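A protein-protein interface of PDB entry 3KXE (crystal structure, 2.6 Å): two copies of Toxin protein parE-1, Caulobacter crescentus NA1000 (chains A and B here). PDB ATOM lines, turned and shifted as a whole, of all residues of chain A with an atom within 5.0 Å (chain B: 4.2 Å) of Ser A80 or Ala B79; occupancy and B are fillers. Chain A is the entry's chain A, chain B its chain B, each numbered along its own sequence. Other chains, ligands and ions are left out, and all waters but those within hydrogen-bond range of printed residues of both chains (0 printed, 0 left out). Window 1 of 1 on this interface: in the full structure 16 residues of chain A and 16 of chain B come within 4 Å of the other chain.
O of Gly A81 lies within hydrogen-bond range of N of Ala B79 (3.0 Å).
The side-chain hydroxyl of Ser B80 lies within hydrogen-bond range of the side-chain hydroxyl of Thr B54, at 2.6 Å.
OH of Tyr A47 sits at hydrogen-bond distance from O of Ser A80.
The side-chain hydroxyl (OG) of Ser A80 is in hydrogen-bond range of the backbone carbonyl oxygen (O) of Glu A50 (3.5 Å).
OG1 of Thr A54 sits close to OG of Ser A80, at 2.9 Å.
Ala B79 touches Ala A79 (CB to CB, 3.7 Å).
O of Ala A79 touches C of Ser B80, 3.7 Å away.
C of Ser A80 touches O of Ala B79 (3.9 Å).
Cys B78 touches Gly A81.
Of the printed residues of chain B, Ser A80 touches Ala B79 (3.9 Å).
Ala B79 touches three residues of chain A.
Of the printed residues of chain A, Cys B78 touches Gly A81 (3.7 Å).
Of the printed residues of chain B, Ala A79 touches Ala B79 and Ser B80.
Printed residues of chain B within 4 Å of Gly A81: Cys B78 and Ala B79.
The nearest printed residue of chain B that does not touch Ser A80 is Ser B80 (4.9 Å).
The nearest printed residue of chain B that does not touch Ala A79 is His B83 (4.9 Å).
Printed residues of chain B that touch a printed residue of chain A: Cys B78, Ala B79 and Ser B80.
Hydrophobic or aromatic side chains of chain B that line the printed part of chain A: Ala B79.
Printed residues of chain A that touch a printed residue of chain B: Ala A79, Ser A80 and Gly A81.
Hydrophobic or aromatic side chains of chain A that line the printed part of chain B: Ala A79.
Ala B79 touches its own counterpart, Ala A79.
Ala A79 touches Ser B80, and with the chains exchanged Ser A80 touches Ala B79.
Positions printed for both chains: 54, 78, 79, 80, 83 and 84.
Of the 5 pairs that touch across the chains among the printed residues, 3 have their exchanged pair printed and touching as well.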
ATOM      1  N   TYR A  47      13.598  15.397   3.722  1.00  0.00           N
ATOM      2  CA  TYR A  47      14.727  15.564   4.635  1.00  0.00           C
ATOM      3  C   TYR A  47      15.402  16.890   4.368  1.00  0.00           C
ATOM      4  O   TYR A  47      15.830  17.570   5.294  1.00  0.00           O
ATOM      5  CB  TYR A  47      15.722  14.409   4.511  1.00  0.00           C
ATOM      6  CG  TYR A  47      16.748  14.288   5.633  1.00  0.00           C
ATOM      7  CD1 TYR A  47      16.469  13.568   6.797  1.00  0.00           C
ATOM      8  CD2 TYR A  47      18.015  14.845   5.506  1.00  0.00           C
ATOM      9  CE1 TYR A  47      17.428  13.431   7.831  1.00  0.00           C
ATOM     10  CE2 TYR A  47      18.990  14.735   6.540  1.00  0.00           C
ATOM     11  CZ  TYR A  47      18.691  14.020   7.687  1.00  0.00           C
ATOM     12  OH  TYR A  47      19.646  13.894   8.667  1.00  0.00           O
ATOM     13  N   GLU A  50      13.818  19.878   5.839  1.00  0.00           N
ATOM     14  CA  GLU A  50      14.146  19.921   7.255  1.00  0.00           C
ATOM     15  C   GLU A  50      15.495  20.584   7.459  1.00  0.00           C
ATOM     16  O   GLU A  50      15.689  21.381   8.391  1.00  0.00           O
ATOM     17  CB  GLU A  50      14.158  18.519   7.843  1.00  0.00           C
ATOM     18  CG  GLU A  50      12.749  17.931   8.034  1.00  0.00           C
ATOM     19  CD  GLU A  50      11.909  18.754   8.974  1.00  0.00           C
ATOM     20  OE1 GLU A  50      10.735  19.059   8.638  1.00  0.00           O
ATOM     21  OE2 GLU A  50      12.436  19.106  10.051  1.00  0.00           O
ATOM     22  N   LEU A  51      16.435  20.288   6.577  1.00  0.00           N
ATOM     23  CA  LEU A  51      17.681  20.988   6.675  1.00  0.00           C
ATOM     24  C   LEU A  51      17.431  22.476   6.404  1.00  0.00           C
ATOM     25  O   LEU A  51      17.957  23.359   7.109  1.00  0.00           O
ATOM     26  CB  LEU A  51      18.730  20.383   5.751  1.00  0.00           C
ATOM     27  CG  LEU A  51      19.291  19.010   6.166  1.00  0.00           C
ATOM     28  CD1 LEU A  51      20.196  18.496   5.079  1.00  0.00           C
ATOM     29  CD2 LEU A  51      20.044  19.060   7.487  1.00  0.00           C
ATOM     30  N   THR A  54      15.913  24.088   9.593  1.00  0.00           N
ATOM     31  CA  THR A  54      16.980  24.254  10.576  1.00  0.00           C
ATOM     32  C   THR A  54      17.822  25.470  10.231  1.00  0.00           C
ATOM     33  O   THR A  54      18.199  26.247  11.107  1.00  0.00           O
ATOM     34  CB  THR A  54      17.966  23.062  10.562  1.00  0.00           C
ATOM     35  OG1 THR A  54      17.249  21.823  10.536  1.00  0.00           O
ATOM     36  CG2 THR A  54      18.922  23.115  11.748  1.00  0.00           C
ATOM     37  N   CYS A  78      23.793  23.341  15.311  1.00  0.00           N
ATOM     38  CA  CYS A  78      22.345  23.170  15.390  1.00  0.00           C
ATOM     39  C   CYS A  78      21.950  21.909  14.599  1.00  0.00           C
ATOM     40  O   CYS A  78      22.132  21.852  13.383  1.00  0.00           O
ATOM     41  CB  CYS A  78      21.656  24.400  14.798  1.00  0.00           C
ATOM     42  SG  CYS A  78      19.862  24.372  14.965  1.00  0.00           S
ATOM     43  N   ALA A  79      21.434  20.897  15.291  1.00  0.00           N
ATOM     44  CA  ALA A  79      21.180  19.580  14.678  1.00  0.00           C
ATOM     45  C   ALA A  79      19.910  19.521  13.841  1.00  0.00           C
ATOM     46  O   ALA A  79      18.940  20.227  14.100  1.00  0.00           O
ATOM     47  CB  ALA A  79      21.157  18.479  15.739  1.00  0.00           C
ATOM     48  N   SER A  80      19.926  18.659  12.837  1.00  0.00           N
ATOM     49  CA  SER A  80      18.748  18.386  12.034  1.00  0.00           C
ATOM     50  C   SER A  80      18.823  16.941  11.573  1.00  0.00           C
ATOM     51  O   SER A  80      19.786  16.536  10.896  1.00  0.00           O
ATOM     52  CB  SER A  80      18.676  19.341  10.851  1.00  0.00           C
ATOM     53  OG  SER A  80      17.637  18.966   9.966  1.00  0.00           O
ATOM     54  N   GLY A  81      17.819  16.163  11.974  1.00  0.00           N
ATOM     55  CA  GLY A  81      17.756  14.731  11.679  1.00  0.00           C
ATOM     56  C   GLY A  81      18.960  13.926  12.166  1.00  0.00           C
ATOM     57  O   GLY A  81      19.154  13.731  13.372  1.00  0.00           O
ATOM     58  N   SER A  82      19.746  13.447  11.203  1.00  0.00           N
ATOM     59  CA  SER A  82      20.968  12.687  11.433  1.00  0.00           C
ATOM     60  C   SER A  82      22.210  13.565  11.298  1.00  0.00           C
ATOM     61  O   SER A  82      23.326  13.081  11.424  1.00  0.00           O
ATOM     62  CB  SER A  82      21.064  11.558  10.410  1.00  0.00           C
ATOM     63  OG  SER A  82      20.291  10.446  10.820  1.00  0.00           O
ATOM     64  N   HIS A  83      21.996  14.851  11.030  1.00  0.00           N
ATOM     65  CA  HIS A  83      23.065  15.783  10.732  1.00  0.00           C
ATOM     66  C   HIS A  83      23.140  16.962  11.676  1.00  0.00           C
ATOM     67  O   HIS A  83      22.252  17.189  12.516  1.00  0.00           O
ATOM     68  CB  HIS A  83      22.911  16.284   9.305  1.00  0.00           C
ATOM     69  CG  HIS A  83      23.228  15.243   8.290  1.00  0.00           C
ATOM     70  ND1 HIS A  83      22.309  14.291   7.891  1.00  0.00           N
ATOM     71  CD2 HIS A  83      24.382  14.951   7.652  1.00  0.00           C
ATOM     72  CE1 HIS A  83      22.881  13.465   7.036  1.00  0.00           C
ATOM     73  NE2 HIS A  83      24.137  13.847   6.868  1.00  0.00           N
ATOM     74  N   VAL A  84      24.219  17.711  11.527  1.00  0.00           N
ATOM     75  CA  VAL A  84      24.524  18.812  12.415  1.00  0.00           C
ATOM     76  C   VAL A  84      24.931  19.976  11.521  1.00  0.00           C
ATOM     77  O   VAL A  84      25.725  19.786  10.605  1.00  0.00           O
ATOM     78  CB  VAL A  84      25.687  18.445  13.379  1.00  0.00           C
ATOM     79  CG1 VAL A  84      26.078  19.646  14.195  1.00  0.00           C
ATOM     80  CG2 VAL A  84      25.310  17.266  14.284  1.00  0.00           C
ATOM     81  N   GLN A 101      26.220  13.558  12.311  1.00  0.00           N
ATOM     82  CA  GLN A 101      26.447  13.447  13.742  1.00  0.00           C
ATOM     83  C   GLN A 101      27.561  12.454  14.098  1.00  0.00           C
ATOM     84  O   GLN A 101      28.028  12.450  15.218  1.00  0.00           O
ATOM     85  CB  GLN A 101      25.145  13.099  14.497  1.00  0.00           C
ATOM     86  CG  GLN A 101      24.666  11.624  14.432  1.00  0.00           C
ATOM     87  CD  GLN A 101      23.114  11.489  14.518  1.00  0.00           C
ATOM     88  OE1 GLN A 101      22.387  12.500  14.546  1.00  0.00           O
ATOM     89  NE2 GLN A 101      22.611  10.235  14.575  1.00  0.00           N
ATOM     90  N   THR B  54      10.069  17.798  13.339  1.00  0.00           N
ATOM     91  CA  THR B  54      10.925  16.635  13.490  1.00  0.00           C
ATOM     92  C   THR B  54      10.067  15.415  13.804  1.00  0.00           C
ATOM     93  O   THR B  54      10.211  14.363  13.161  1.00  0.00           O
ATOM     94  CB  THR B  54      11.973  16.882  14.596  1.00  0.00           C
ATOM     95  OG1 THR B  54      12.761  18.036  14.255  1.00  0.00           O
ATOM     96  CG2 THR B  54      12.883  15.674  14.779  1.00  0.00           C
ATOM     97  N   CYS B  78      16.221  11.025  16.370  1.00  0.00           N
ATOM     98  CA  CYS B  78      16.175  12.057  15.361  1.00  0.00           C
ATOM     99  C   CYS B  78      16.378  13.345  16.108  1.00  0.00           C
ATOM    100  O   CYS B  78      15.603  13.696  16.978  1.00  0.00           O
ATOM    101  CB  CYS B  78      14.831  12.067  14.649  1.00  0.00           C
ATOM    102  SG  CYS B  78      14.916  12.866  13.083  1.00  0.00           S
ATOM    103  N   ALA B  79      17.465  14.023  15.814  1.00  0.00           N
ATOM    104  CA  ALA B  79      17.797  15.216  16.556  1.00  0.00           C
ATOM    105  C   ALA B  79      17.074  16.426  15.935  1.00  0.00           C
ATOM    106  O   ALA B  79      16.607  16.388  14.788  1.00  0.00           O
ATOM    107  CB  ALA B  79      19.297  15.407  16.570  1.00  0.00           C
ATOM    108  N   SER B  80      16.985  17.499  16.708  1.00  0.00           N
ATOM    109  CA  SER B  80      16.263  18.682  16.285  1.00  0.00           C
ATOM    110  C   SER B  80      16.768  19.825  17.120  1.00  0.00           C
ATOM    111  O   SER B  80      16.566  19.827  18.334  1.00  0.00           O
ATOM    112  CB  SER B  80      14.774  18.503  16.515  1.00  0.00           C
ATOM    113  OG  SER B  80      14.108  19.583  15.928  1.00  0.00           O
ATOM    114  N   HIS B  83      18.125  19.503  20.612  1.00  0.00           N
ATOM    115  CA  HIS B  83      17.519  18.333  21.199  1.00  0.00           C
ATOM    116  C   HIS B  83      17.594  17.030  20.380  1.00  0.00           C
ATOM    117  O   HIS B  83      18.096  17.016  19.243  1.00  0.00           O
ATOM    118  CB  HIS B  83      16.122  18.664  21.729  1.00  0.00           C
ATOM    119  CG  HIS B  83      16.170  19.572  22.916  1.00  0.00           C
ATOM    120  ND1 HIS B  83      16.184  20.949  22.802  1.00  0.00           N
ATOM    121  CD2 HIS B  83      16.303  19.296  24.235  1.00  0.00           C
ATOM    122  CE1 HIS B  83      16.293  21.480  24.003  1.00  0.00           C
ATOM    123  NE2 HIS B  83      16.366  20.501  24.891  1.00  0.00           N
ATOM    124  N   VAL B  84      17.131  15.942  21.008  1.00  0.00           N
ATOM    125  CA  VAL B  84      17.149  14.604  20.410  1.00  0.00           C
ATOM    126  C   VAL B  84      15.888  13.861  20.808  1.00  0.00           C
ATOM    127  O   VAL B  84      15.680  13.582  21.993  1.00  0.00           O
ATOM    128  CB  VAL B  84      18.376  13.752  20.850  1.00  0.00           C
ATOM    129  CG1 VAL B  84      18.406  12.490  20.052  1.00  0.00           C
ATOM    130  CG2 VAL B  84      19.673  14.509  20.676  1.00  0.00           C
